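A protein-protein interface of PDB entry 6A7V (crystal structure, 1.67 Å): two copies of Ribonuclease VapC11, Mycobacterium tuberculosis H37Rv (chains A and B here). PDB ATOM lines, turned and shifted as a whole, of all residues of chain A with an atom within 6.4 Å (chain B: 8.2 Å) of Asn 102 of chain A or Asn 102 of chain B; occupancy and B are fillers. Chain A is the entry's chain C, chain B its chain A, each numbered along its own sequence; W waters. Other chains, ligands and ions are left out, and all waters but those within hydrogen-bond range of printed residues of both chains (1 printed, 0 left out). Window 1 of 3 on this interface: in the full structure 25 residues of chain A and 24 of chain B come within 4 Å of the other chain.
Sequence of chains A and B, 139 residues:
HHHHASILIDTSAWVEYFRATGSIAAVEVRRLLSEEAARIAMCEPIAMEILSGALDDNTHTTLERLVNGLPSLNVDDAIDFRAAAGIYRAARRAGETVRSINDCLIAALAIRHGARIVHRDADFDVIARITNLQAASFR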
ATOM      1  N   PRO A  45       1.367  -3.984 -30.357  1.00  0.00           N
ATOM      2  CA  PRO A  45       0.507  -3.189 -29.535  1.00  0.00           C
ATOM      3  C   PRO A  45      -0.951  -3.685 -29.606  1.00  0.00           C
ATOM      4  O   PRO A  45      -1.647  -3.745 -28.613  1.00  0.00           O
ATOM      5  CB  PRO A  45       0.648  -1.784 -30.119  1.00  0.00           C
ATOM      6  CG  PRO A  45       2.046  -1.757 -30.657  1.00  0.00           C
ATOM      7  CD  PRO A  45       2.262  -3.147 -31.186  1.00  0.00           C
ATOM      8  N   MET A  48      -1.241  -6.980 -27.604  1.00  0.00           N
ATOM      9  CA  MET A  48      -1.274  -6.706 -26.166  1.00  0.00           C
ATOM     10  C   MET A  48      -2.670  -6.321 -25.731  1.00  0.00           C
ATOM     11  O   MET A  48      -3.171  -6.853 -24.714  1.00  0.00           O
ATOM     12  CB  MET A  48      -0.309  -5.563 -25.850  1.00  0.00           C
ATOM     13  CG  MET A  48      -0.333  -5.082 -24.405  1.00  0.00           C
ATOM     14  SD  MET A  48       0.837  -3.741 -24.122  1.00  0.00           S
ATOM     15  CE  MET A  48       0.055  -2.413 -25.037  1.00  0.00           C
ATOM     16  N   GLU A  49      -3.328  -5.473 -26.515  1.00  0.00           N
ATOM     17  CA  GLU A  49      -4.693  -5.059 -26.233  1.00  0.00           C
ATOM     18  C   GLU A  49      -5.686  -6.254 -26.280  1.00  0.00           C
ATOM     19  O   GLU A  49      -6.469  -6.464 -25.378  1.00  0.00           O
ATOM     20  CB  GLU A  49      -5.159  -3.930 -27.153  1.00  0.00           C
ATOM     21  CG  GLU A  49      -4.453  -2.608 -26.902  1.00  0.00           C
ATOM     22  CD  GLU A  49      -4.912  -1.511 -27.845  1.00  0.00           C
ATOM     23  OE1 GLU A  49      -5.318  -1.831 -28.982  1.00  0.00           O
ATOM     24  OE2 GLU A  49      -4.866  -0.325 -27.449  1.00  0.00           O
ATOM     25  N   PHE A  81       8.261   5.222 -31.457  1.00  0.00           N
ATOM     26  CA  PHE A  81       7.770   5.945 -30.309  1.00  0.00           C
ATOM     27  C   PHE A  81       7.845   7.461 -30.514  1.00  0.00           C
ATOM     28  O   PHE A  81       6.870   8.169 -30.227  1.00  0.00           O
ATOM     29  CB  PHE A  81       8.458   5.480 -29.026  1.00  0.00           C
ATOM     30  CG  PHE A  81       8.086   4.080 -28.640  1.00  0.00           C
ATOM     31  CD1 PHE A  81       6.940   3.832 -27.886  1.00  0.00           C
ATOM     32  CD2 PHE A  81       8.845   3.004 -29.060  1.00  0.00           C
ATOM     33  CE1 PHE A  81       6.580   2.537 -27.545  1.00  0.00           C
ATOM     34  CE2 PHE A  81       8.492   1.706 -28.721  1.00  0.00           C
ATOM     35  CZ  PHE A  81       7.360   1.475 -27.961  1.00  0.00           C
ATOM     36  N   SER A 100      -6.203   7.638 -27.136  1.00  0.00           N
ATOM     37  CA  SER A 100      -5.143   6.710 -26.753  1.00  0.00           C
ATOM     38  C   SER A 100      -3.847   6.988 -27.525  1.00  0.00           C
ATOM     39  O   SER A 100      -3.844   6.976 -28.751  1.00  0.00           O
ATOM     40  CB  SER A 100      -5.614   5.279 -27.023  1.00  0.00           C
ATOM     41  OG  SER A 100      -4.617   4.316 -26.728  1.00  0.00           O
ATOM     42  N   ILE A 101      -2.752   7.229 -26.803  1.00  0.00           N
ATOM     43  CA  ILE A 101      -1.460   7.370 -27.396  1.00  0.00           C
ATOM     44  C   ILE A 101      -0.986   6.081 -28.045  1.00  0.00           C
ATOM     45  O   ILE A 101      -0.198   6.160 -28.960  1.00  0.00           O
ATOM     46  CB  ILE A 101      -0.416   7.908 -26.389  1.00  0.00           C
ATOM     47  CG1 ILE A 101       0.819   8.396 -27.154  1.00  0.00           C
ATOM     48  CG2 ILE A 101      -0.067   6.851 -25.346  1.00  0.00           C
ATOM     49  CD1 ILE A 101       1.555   9.525 -26.482  1.00  0.00           C
ATOM     50  N   ASN A 102      -1.503   4.925 -27.646  1.00  0.00           N
ATOM     51  CA  ASN A 102      -1.185   3.706 -28.379  1.00  0.00           C
ATOM     52  C   ASN A 102      -1.851   3.682 -29.731  1.00  0.00           C
ATOM     53  O   ASN A 102      -1.240   3.112 -30.619  1.00  0.00           O
ATOM     54  CB  ASN A 102      -1.466   2.453 -27.553  1.00  0.00           C
ATOM     55  CG  ASN A 102      -0.403   2.219 -26.492  1.00  0.00           C
ATOM     56  OD1 ASN A 102       0.705   2.777 -26.565  1.00  0.00           O
ATOM     57  ND2 ASN A 102      -0.725   1.390 -25.503  1.00  0.00           N
ATOM     58  N   ASP A 103      -2.940   4.409 -29.955  1.00  0.00           N
ATOM     59  CA  ASP A 103      -3.434   4.556 -31.328  1.00  0.00           C
ATOM     60  C   ASP A 103      -2.432   5.319 -32.192  1.00  0.00           C
ATOM     61  O   ASP A 103      -2.193   4.938 -33.316  1.00  0.00           O
ATOM     62  CB  ASP A 103      -4.821   5.186 -31.375  1.00  0.00           C
ATOM     63  CG  ASP A 103      -5.881   4.254 -30.842  1.00  0.00           C
ATOM     64  OD1 ASP A 103      -5.621   3.035 -30.830  1.00  0.00           O
ATOM     65  OD2 ASP A 103      -6.962   4.723 -30.431  1.00  0.00           O
ATOM     66  N   CYS A 104      -1.800   6.316 -31.655  1.00  0.00           N
ATOM     67  CA  CYS A 104      -0.746   7.033 -32.360  1.00  0.00           C
ATOM     68  C   CYS A 104       0.433   6.125 -32.663  1.00  0.00           C
ATOM     69  O   CYS A 104       0.931   6.177 -33.800  1.00  0.00           O
ATOM     70  CB  CYS A 104      -0.237   8.235 -31.559  1.00  0.00           C
ATOM     71  SG  CYS A 104      -1.472   9.512 -31.299  1.00  0.00           S
ATOM     72  N   LEU A 105       0.811   5.245 -31.759  1.00  0.00           N
ATOM     73  CA  LEU A 105       1.845   4.284 -31.974  1.00  0.00           C
ATOM     74  C   LEU A 105       1.506   3.336 -33.124  1.00  0.00           C
ATOM     75  O   LEU A 105       2.354   3.109 -34.033  1.00  0.00           O
ATOM     76  CB  LEU A 105       2.139   3.472 -30.707  1.00  0.00           C
ATOM     77  CG  LEU A 105       3.280   2.445 -30.801  1.00  0.00           C
ATOM     78  CD1 LEU A 105       4.611   3.086 -31.170  1.00  0.00           C
ATOM     79  CD2 LEU A 105       3.402   1.696 -29.479  1.00  0.00           C
ATOM     80  N   ILE A 106       0.298   2.793 -33.072  1.00  0.00           N
ATOM     81  CA  ILE A 106      -0.203   1.884 -34.073  1.00  0.00           C
ATOM     82  C   ILE A 106      -0.168   2.561 -35.454  1.00  0.00           C
ATOM     83  O   ILE A 106       0.289   1.970 -36.457  1.00  0.00           O
ATOM     84  CB  ILE A 106      -1.643   1.405 -33.726  1.00  0.00           C
ATOM     85  CG1 ILE A 106      -1.604   0.452 -32.527  1.00  0.00           C
ATOM     86  CG2 ILE A 106      -2.308   0.698 -34.904  1.00  0.00           C
ATOM     87  CD1 ILE A 106      -2.937   0.248 -31.826  1.00  0.00           C
ATOM     88  N   ALA A 107      -0.649   3.782 -35.493  1.00  0.00           N
ATOM     89  CA  ALA A 107      -0.689   4.529 -36.752  1.00  0.00           C
ATOM     90  C   ALA A 107       0.694   4.794 -37.272  1.00  0.00           C
ATOM     91  O   ALA A 107       0.913   4.625 -38.474  1.00  0.00           O
ATOM     92  CB  ALA A 107      -1.401   5.851 -36.539  1.00  0.00           C
ATOM     93  N   PHE A 124      -8.286   7.226 -35.242  1.00  0.00           N
ATOM     94  CA  PHE A 124      -7.675   7.014 -36.565  1.00  0.00           C
ATOM     95  C   PHE A 124      -8.179   7.968 -37.626  1.00  0.00           C
ATOM     96  O   PHE A 124      -7.416   8.422 -38.474  1.00  0.00           O
ATOM     97  CB  PHE A 124      -7.797   5.567 -37.005  1.00  0.00           C
ATOM     98  CG  PHE A 124      -7.071   4.632 -36.102  1.00  0.00           C
ATOM     99  CD1 PHE A 124      -5.689   4.623 -36.080  1.00  0.00           C
ATOM    100  CD2 PHE A 124      -7.759   3.795 -35.242  1.00  0.00           C
ATOM    101  CE1 PHE A 124      -5.000   3.776 -35.231  1.00  0.00           C
ATOM    102  CE2 PHE A 124      -7.077   2.951 -34.392  1.00  0.00           C
ATOM    103  CZ  PHE A 124      -5.693   2.937 -34.387  1.00  0.00           C
ATOM    104  N   ASP B  10      10.285   7.055 -13.847  1.00  0.00           N
ATOM    105  CA  ASP B  10       8.990   7.049 -14.516  1.00  0.00           C
ATOM    106  C   ASP B  10       8.534   8.459 -14.861  1.00  0.00           C
ATOM    107  O   ASP B  10       8.936   9.418 -14.219  1.00  0.00           O
ATOM    108  CB  ASP B  10       7.930   6.392 -13.635  1.00  0.00           C
ATOM    109  CG  ASP B  10       6.602   6.243 -14.348  1.00  0.00           C
ATOM    110  OD1 ASP B  10       6.587   5.653 -15.455  1.00  0.00           O
ATOM    111  OD2 ASP B  10       5.574   6.737 -13.825  1.00  0.00           O
ATOM    112  N   CYS B  43      13.668   4.908 -21.460  1.00  0.00           N
ATOM    113  CA  CYS B  43      13.163   3.967 -22.445  1.00  0.00           C
ATOM    114  C   CYS B  43      12.180   4.698 -23.325  1.00  0.00           C
ATOM    115  O   CYS B  43      11.677   5.779 -22.973  1.00  0.00           O
ATOM    116  CB  CYS B  43      12.525   2.736 -21.800  1.00  0.00           C
ATOM    117  SG  CYS B  43      10.991   3.009 -20.900  1.00  0.00           S
ATOM    118  N   PRO B  45       9.038   4.108 -24.333  1.00  0.00           N
ATOM    119  CA  PRO B  45       7.683   4.394 -23.925  1.00  0.00           C
ATOM    120  C   PRO B  45       7.619   5.608 -22.982  1.00  0.00           C
ATOM    121  O   PRO B  45       6.751   6.435 -23.094  1.00  0.00           O
ATOM    122  CB  PRO B  45       7.254   3.106 -23.220  1.00  0.00           C
ATOM    123  CG  PRO B  45       8.017   2.043 -23.926  1.00  0.00           C
ATOM    124  CD  PRO B  45       9.349   2.670 -24.253  1.00  0.00           C
ATOM    125  N   ILE B  46       8.585   5.716 -22.088  1.00  0.00           N
ATOM    126  CA  ILE B  46       8.643   6.888 -21.227  1.00  0.00           C
ATOM    127  C   ILE B  46       8.894   8.174 -22.032  1.00  0.00           C
ATOM    128  O   ILE B  46       8.271   9.185 -21.805  1.00  0.00           O
ATOM    129  CB  ILE B  46       9.675   6.721 -20.094  1.00  0.00           C
ATOM    130  CG1 ILE B  46       9.158   5.661 -19.111  1.00  0.00           C
ATOM    131  CG2 ILE B  46       9.913   8.045 -19.375  1.00  0.00           C
ATOM    132  CD1 ILE B  46      10.107   5.333 -17.974  1.00  0.00           C
ATOM    133  N   MET B  48       8.193   8.788 -25.176  1.00  0.00           N
ATOM    134  CA  MET B  48       6.986   9.136 -25.914  1.00  0.00           C
ATOM    135  C   MET B  48       6.017   9.917 -25.026  1.00  0.00           C
ATOM    136  O   MET B  48       5.493  10.959 -25.433  1.00  0.00           O
ATOM    137  CB  MET B  48       6.321   7.854 -26.427  1.00  0.00           C
ATOM    138  CG  MET B  48       4.962   8.053 -27.077  1.00  0.00           C
ATOM    139  SD  MET B  48       4.175   6.499 -27.549  1.00  0.00           S
ATOM    140  CE  MET B  48       3.756   5.806 -25.949  1.00  0.00           C
ATOM    141  N   GLU B  49       5.869   9.467 -23.783  1.00  0.00           N
ATOM    142  CA  GLU B  49       4.992  10.137 -22.846  1.00  0.00           C
ATOM    143  C   GLU B  49       5.496  11.564 -22.555  1.00  0.00           C
ATOM    144  O   GLU B  49       4.757  12.532 -22.547  1.00  0.00           O
ATOM    145  CB  GLU B  49       4.829   9.339 -21.548  1.00  0.00           C
ATOM    146  CG  GLU B  49       4.050   8.056 -21.747  1.00  0.00           C
ATOM    147  CD  GLU B  49       3.842   7.270 -20.472  1.00  0.00           C
ATOM    148  OE1 GLU B  49       4.613   7.457 -19.506  1.00  0.00           O
ATOM    149  OE2 GLU B  49       2.901   6.450 -20.448  1.00  0.00           O
ATOM    150  N   PHE B  81       5.591  -6.627 -25.145  1.00  0.00           N
ATOM    151  CA  PHE B  81       4.176  -6.408 -25.180  1.00  0.00           C
ATOM    152  C   PHE B  81       3.400  -7.596 -24.596  1.00  0.00           C
ATOM    153  O   PHE B  81       2.435  -7.417 -23.881  1.00  0.00           O
ATOM    154  CB  PHE B  81       3.725  -6.067 -26.607  1.00  0.00           C
ATOM    155  CG  PHE B  81       4.275  -4.761 -27.112  1.00  0.00           C
ATOM    156  CD1 PHE B  81       3.609  -3.571 -26.863  1.00  0.00           C
ATOM    157  CD2 PHE B  81       5.466  -4.720 -27.829  1.00  0.00           C
ATOM    158  CE1 PHE B  81       4.124  -2.361 -27.311  1.00  0.00           C
ATOM    159  CE2 PHE B  81       5.980  -3.518 -28.288  1.00  0.00           C
ATOM    160  CZ  PHE B  81       5.305  -2.336 -28.027  1.00  0.00           C
ATOM    161  N   ALA B  84       3.712  -7.466 -20.872  1.00  0.00           N
ATOM    162  CA  ALA B  84       2.836  -6.406 -20.345  1.00  0.00           C
ATOM    163  C   ALA B  84       1.414  -6.912 -20.266  1.00  0.00           C
ATOM    164  O   ALA B  84       0.742  -6.683 -19.246  1.00  0.00           O
ATOM    165  CB  ALA B  84       2.897  -5.183 -21.248  1.00  0.00           C
ATOM    166  N   TYR B  88      -0.944  -7.353 -16.971  1.00  0.00           N
ATOM    167  CA  TYR B  88      -2.264  -6.736 -16.915  1.00  0.00           C
ATOM    168  C   TYR B  88      -3.289  -7.780 -16.460  1.00  0.00           C
ATOM    169  O   TYR B  88      -4.140  -7.510 -15.567  1.00  0.00           O
ATOM    170  CB  TYR B  88      -2.656  -6.137 -18.272  1.00  0.00           C
ATOM    171  CG  TYR B  88      -3.892  -5.265 -18.229  1.00  0.00           C
ATOM    172  CD1 TYR B  88      -3.794  -3.903 -17.963  1.00  0.00           C
ATOM    173  CD2 TYR B  88      -5.158  -5.798 -18.455  1.00  0.00           C
ATOM    174  CE1 TYR B  88      -4.918  -3.096 -17.920  1.00  0.00           C
ATOM    175  CE2 TYR B  88      -6.288  -4.998 -18.413  1.00  0.00           C
ATOM    176  CZ  TYR B  88      -6.162  -3.645 -18.147  1.00  0.00           C
ATOM    177  OH  TYR B  88      -7.272  -2.835 -18.105  1.00  0.00           O
ATOM    178  N   VAL B  98      -5.425  -1.369 -12.961  1.00  0.00           N
ATOM    179  CA  VAL B  98      -4.269  -0.774 -13.620  1.00  0.00           C
ATOM    180  C   VAL B  98      -4.791   0.342 -14.507  1.00  0.00           C
ATOM    181  O   VAL B  98      -5.618   0.104 -15.382  1.00  0.00           O
ATOM    182  CB  VAL B  98      -3.499  -1.806 -14.466  1.00  0.00           C
ATOM    183  CG1 VAL B  98      -2.352  -1.139 -15.215  1.00  0.00           C
ATOM    184  CG2 VAL B  98      -2.976  -2.930 -13.583  1.00  0.00           C
ATOM    185  N   ARG B  99      -4.320   1.562 -14.271  1.00  0.00           N
ATOM    186  CA  ARG B  99      -4.808   2.718 -15.017  1.00  0.00           C
ATOM    187  C   ARG B  99      -4.241   2.800 -16.433  1.00  0.00           C
ATOM    188  O   ARG B  99      -4.944   3.228 -17.345  1.00  0.00           O
ATOM    189  CB  ARG B  99      -4.537   4.009 -14.249  1.00  0.00           C
ATOM    190  CG  ARG B  99      -5.430   4.153 -13.024  1.00  0.00           C
ATOM    191  CD  ARG B  99      -5.278   5.505 -12.346  1.00  0.00           C
ATOM    192  NE  ARG B  99      -4.107   5.555 -11.471  1.00  0.00           N
ATOM    193  CZ  ARG B  99      -2.891   5.972 -11.825  1.00  0.00           C
ATOM    194  NH1 ARG B  99      -1.923   5.959 -10.920  1.00  0.00           N
ATOM    195  NH2 ARG B  99      -2.626   6.401 -13.059  1.00  0.00           N
ATOM    196  N   SER B 100      -2.988   2.390 -16.613  1.00  0.00           N
ATOM    197  CA  SER B 100      -2.330   2.456 -17.927  1.00  0.00           C
ATOM    198  C   SER B 100      -1.630   1.150 -18.312  1.00  0.00           C
ATOM    199  O   SER B 100      -0.731   0.698 -17.611  1.00  0.00           O
ATOM    200  CB  SER B 100      -1.315   3.598 -17.934  1.00  0.00           C
ATOM    201  OG  SER B 100      -0.654   3.700 -19.181  1.00  0.00           O
ATOM    202  N   ILE B 101      -2.034   0.567 -19.442  1.00  0.00           N
ATOM    203  CA  ILE B 101      -1.385  -0.590 -20.014  1.00  0.00           C
ATOM    204  C   ILE B 101       0.063  -0.301 -20.353  1.00  0.00           C
ATOM    205  O   ILE B 101       0.857  -1.212 -20.304  1.00  0.00           O
ATOM    206  CB  ILE B 101      -2.167  -1.125 -21.250  1.00  0.00           C
ATOM    207  CG1 ILE B 101      -1.605  -2.462 -21.749  1.00  0.00           C
ATOM    208  CG2 ILE B 101      -2.158  -0.118 -22.393  1.00  0.00           C
ATOM    209  CD1 ILE B 101      -1.797  -3.625 -20.806  1.00  0.00           C
ATOM    210  N   ASN B 102       0.422   0.945 -20.653  1.00  0.00           N
ATOM    211  CA  ASN B 102       1.812   1.283 -20.885  1.00  0.00           C
ATOM    212  C   ASN B 102       2.625   1.258 -19.619  1.00  0.00           C
ATOM    213  O   ASN B 102       3.803   0.929 -19.733  1.00  0.00           O
ATOM    214  CB  ASN B 102       1.939   2.596 -21.667  1.00  0.00           C
ATOM    215  CG  ASN B 102       1.607   2.410 -23.139  1.00  0.00           C
ATOM    216  OD1 ASN B 102       1.504   1.274 -23.617  1.00  0.00           O
ATOM    217  ND2 ASN B 102       1.428   3.512 -23.865  1.00  0.00           N
ATOM    218  N   ASP B 103       2.006   1.390 -18.443  1.00  0.00           N
ATOM    219  CA  ASP B 103       2.748   1.119 -17.199  1.00  0.00           C
ATOM    220  C   ASP B 103       3.156  -0.340 -17.123  1.00  0.00           C
ATOM    221  O   ASP B 103       4.282  -0.626 -16.750  1.00  0.00           O
ATOM    222  CB  ASP B 103       1.968   1.579 -15.970  1.00  0.00           C
ATOM    223  CG  ASP B 103       1.909   3.089 -15.866  1.00  0.00           C
ATOM    224  OD1 ASP B 103       2.741   3.759 -16.511  1.00  0.00           O
ATOM    225  OD2 ASP B 103       1.046   3.617 -15.138  1.00  0.00           O
ATOM    226  N   CYS B 104       2.331  -1.254 -17.574  1.00  0.00           N
ATOM    227  CA  CYS B 104       2.676  -2.660 -17.632  1.00  0.00           C
ATOM    228  C   CYS B 104       3.796  -2.931 -18.635  1.00  0.00           C
ATOM    229  O   CYS B 104       4.685  -3.715 -18.330  1.00  0.00           O
ATOM    230  CB  CYS B 104       1.461  -3.489 -18.062  1.00  0.00           C
ATOM    231  SG  CYS B 104       0.083  -3.488 -16.893  1.00  0.00           S
ATOM    232  N   LEU B 105       3.826  -2.235 -19.730  1.00  0.00           N
ATOM    233  CA  LEU B 105       4.875  -2.333 -20.713  1.00  0.00           C
ATOM    234  C   LEU B 105       6.220  -1.890 -20.124  1.00  0.00           C
ATOM    235  O   LEU B 105       7.249  -2.601 -20.251  1.00  0.00           O
ATOM    236  CB  LEU B 105       4.556  -1.509 -21.966  1.00  0.00           C
ATOM    237  CG  LEU B 105       5.624  -1.482 -23.066  1.00  0.00           C
ATOM    238  CD1 LEU B 105       5.886  -2.875 -23.622  1.00  0.00           C
ATOM    239  CD2 LEU B 105       5.202  -0.536 -24.174  1.00  0.00           C
ATOM    240  N   ILE B 106       6.179  -0.734 -19.482  1.00  0.00           N
ATOM    241  CA  ILE B 106       7.351  -0.147 -18.851  1.00  0.00           C
ATOM    242  C   ILE B 106       7.883  -1.117 -17.780  1.00  0.00           C
ATOM    243  O   ILE B 106       9.100  -1.354 -17.696  1.00  0.00           O
ATOM    244  CB  ILE B 106       7.025   1.238 -18.225  1.00  0.00           C
ATOM    245  CG1 ILE B 106       6.830   2.277 -19.335  1.00  0.00           C
ATOM    246  CG2 ILE B 106       8.133   1.708 -17.289  1.00  0.00           C
ATOM    247  CD1 ILE B 106       6.105   3.530 -18.903  1.00  0.00           C
ATOM    248  N   ALA B 107       6.991  -1.662 -16.988  1.00  0.00           N
ATOM    249  CA  ALA B 107       7.427  -2.580 -15.938  1.00  0.00           C
ATOM    250  C   ALA B 107       8.007  -3.838 -16.519  1.00  0.00           C
ATOM    251  O   ALA B 107       9.027  -4.291 -15.996  1.00  0.00           O
ATOM    252  CB  ALA B 107       6.247  -2.923 -15.032  1.00  0.00           C
ATOM    253  N   ALA B 108       7.451  -4.341 -17.610  1.00  0.00           N
ATOM    254  CA  ALA B 108       8.020  -5.495 -18.299  1.00  0.00           C
ATOM    255  C   ALA B 108       9.436  -5.210 -18.731  1.00  0.00           C
ATOM    256  O   ALA B 108      10.330  -6.060 -18.576  1.00  0.00           O
ATOM    257  CB  ALA B 108       7.160  -5.891 -19.496  1.00  0.00           C
ATOM    258  N   LEU B 109       9.614  -4.024 -19.332  1.00  0.00           N
ATOM    259  CA  LEU B 109      10.909  -3.579 -19.822  1.00  0.00           C
ATOM    260  C   LEU B 109      11.934  -3.581 -18.670  1.00  0.00           C
ATOM    261  O   LEU B 109      13.067  -4.079 -18.778  1.00  0.00           O
ATOM    262  CB  LEU B 109      10.731  -2.209 -20.493  1.00  0.00           C
ATOM    263  CG  LEU B 109      11.870  -1.577 -21.268  1.00  0.00           C
ATOM    264  CD1 LEU B 109      11.308  -0.744 -22.410  1.00  0.00           C
ATOM    265  CD2 LEU B 109      12.717  -0.727 -20.338  1.00  0.00           C
ATOM    266  N   ILE B 117      12.683   1.100 -10.976  1.00  0.00           N
ATOM    267  CA  ILE B 117      11.870   2.220 -11.424  1.00  0.00           C
ATOM    268  C   ILE B 117      11.492   3.115 -10.248  1.00  0.00           C
ATOM    269  O   ILE B 117      10.999   2.637  -9.212  1.00  0.00           O
ATOM    270  CB  ILE B 117      10.610   1.755 -12.207  1.00  0.00           C
ATOM    271  CG1 ILE B 117       9.789   2.962 -12.668  1.00  0.00           C
ATOM    272  CG2 ILE B 117       9.742   0.819 -11.389  1.00  0.00           C
ATOM    273  CD1 ILE B 117       8.987   2.691 -13.924  1.00  0.00           C
ATOM    274  N   ASP B 123       0.156   2.257 -10.149  1.00  0.00           N
ATOM    275  CA  ASP B 123       0.270   1.128 -11.066  1.00  0.00           C
ATOM    276  C   ASP B 123       1.535   0.335 -10.741  1.00  0.00           C
ATOM    277  O   ASP B 123       1.506  -0.899 -10.724  1.00  0.00           O
ATOM    278  CB  ASP B 123       0.348   1.599 -12.527  1.00  0.00           C
ATOM    279  CG  ASP B 123      -1.005   1.939 -13.120  1.00  0.00           C
ATOM    280  OD1 ASP B 123      -2.027   1.838 -12.409  1.00  0.00           O
ATOM    281  OD2 ASP B 123      -1.050   2.291 -14.323  1.00  0.00           O
ATOM    282  N   PHE B 124       2.671   0.993 -10.504  1.00  0.00           N
ATOM    283  CA  PHE B 124       3.866   0.296 -10.190  1.00  0.00           C
ATOM    284  C   PHE B 124       3.840  -0.381  -8.854  1.00  0.00           C
ATOM    285  O   PHE B 124       4.399  -1.484  -8.728  1.00  0.00           O
ATOM    286  CB  PHE B 124       5.070   1.206 -10.356  1.00  0.00           C
ATOM    287  CG  PHE B 124       5.211   1.695 -11.756  1.00  0.00           C
ATOM    288  CD1 PHE B 124       5.527   0.806 -12.762  1.00  0.00           C
ATOM    289  CD2 PHE B 124       4.951   3.016 -12.077  1.00  0.00           C
ATOM    290  CE1 PHE B 124       5.624   1.232 -14.074  1.00  0.00           C
ATOM    291  CE2 PHE B 124       5.048   3.449 -13.384  1.00  0.00           C
ATOM    292  CZ  PHE B 124       5.385   2.558 -14.379  1.00  0.00           C
ATOM    293  N   ILE B 127       2.038  -3.539  -9.603  1.00  0.00           N
ATOM    294  CA  ILE B 127       2.799  -4.460 -10.389  1.00  0.00           C
ATOM    295  C   ILE B 127       3.910  -5.086  -9.565  1.00  0.00           C
ATOM    296  O   ILE B 127       4.216  -6.259  -9.831  1.00  0.00           O
ATOM    297  CB  ILE B 127       3.347  -3.794 -11.684  1.00  0.00           C
ATOM    298  CG1 ILE B 127       2.179  -3.414 -12.602  1.00  0.00           C
ATOM    299  CG2 ILE B 127       4.286  -4.735 -12.433  1.00  0.00           C
ATOM    300  CD1 ILE B 127       2.538  -2.454 -13.711  1.00  0.00           C
HETATM  301  O   HOH W   1       2.943   1.272 -26.007  1.00  0.00           O
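Printed residues of chain A that touch a printed residue of chain B: Pro 45, Met 48, Phe 81, Ile 101 and Asn 102. Of the 25 printed residues of chain B, 6 touch a printed residue of chain A. Hydrophobic or aromatic side chains of chain B that line the printed part of chain A: Pro 45, Met 48, Phe 81, Ala 84 and Ile 101. Among the printed residues, 10 pairs touch across the chains. Among the printed residues, no Asp or Glu carboxylate lies within 4 Å of a Lys or Arg side-chain nitrogen of the other chain.
The side-chain hydroxyl (OG) of Ser 100 of chain B lies close to the backbone NH (N) of Asn 102 of chain B, 3.3 Å away. OG of Ser 100 of chain A sits close to N of Asn 102 of chain A.
Water W1 lies within hydrogen-bond range of OD1 of Asn 102 of chain A and OD1 of Asn 102 of chain B.
Printed residues of chain B within 4 Å of Met 48 of chain A: Phe 81, Ala 84 and Ile 101. Of the printed residues of chain B, Ile 101 of chain A touches Met 48 (3.8 Å) and Asn 102 (3.9 Å). Of chain B, only Ile 101 and Asn 102 come within 4 Å of Asn 102 of chain A. Printed residues of chain A within 4 Å of Met 48 of chain B: Phe 81 and Ile 101. Asn 102 of chain B touches just these residues of chain A: Ile 101 (3.9 Å) and Asn 102 (2.9 Å). The nearest residue of chain B that does not touch Asn 102 of chain A is Met 48 of chain B (4.3 Å). The nearest residue of chain A that does not touch Asn 102 of chain B is Met 48 of chain A (4.2 Å).
Pro 45 of chain A touches Phe 81 of chain B, and with the chains exchanged Phe 81 of chain A touches Pro 45 of chain B. Met 48 of chain A touches Phe 81 of chain B, and with the chains exchanged Phe 81 of chain A touches Met 48 of chain B. Met 48 of chain A touches Ile 101 of chain B, and with the chains exchanged Ile 101 of chain A touches Met 48 of chain B. Ile 101 of chain A touches Asn 102 of chain B, and with the chains exchanged Asn 102 of chain A touches Ile 101 of chain B. Of the 10 pairs that touch across the chains among the printed residues, 9 have their exchanged pair printed and touching as well.
Among the printed residues, pairs that only touch across the chains: Met 48 of chain A with Ile 101 of chain B (3.6 Å), Met 48 of chain A with Phe 81 of chain B (3.7 Å), Phe 81 of chain A with Met 48 of chain B (3.7 Å), Asn 102 of chain A with Ile 101 of chain B (3.7 Å), Ile 101 of chain A with Met 48 of chain B (3.8 Å), Met 48 of chain A with Ala 84 of chain B (3.8 Å), Phe 81 of chain A with Pro 45 of chain B (3.9 Å), Ile 101 of chain A with Asn 102 of chain B (3.9 Å) and Pro 45 of chain A with Phe 81 of chain B (3.98 Å).
OD1 of Asn 102 of chain A sits at hydrogen-bond distance from ND2 of Asn 102 of chain B, 2.9 Å away.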
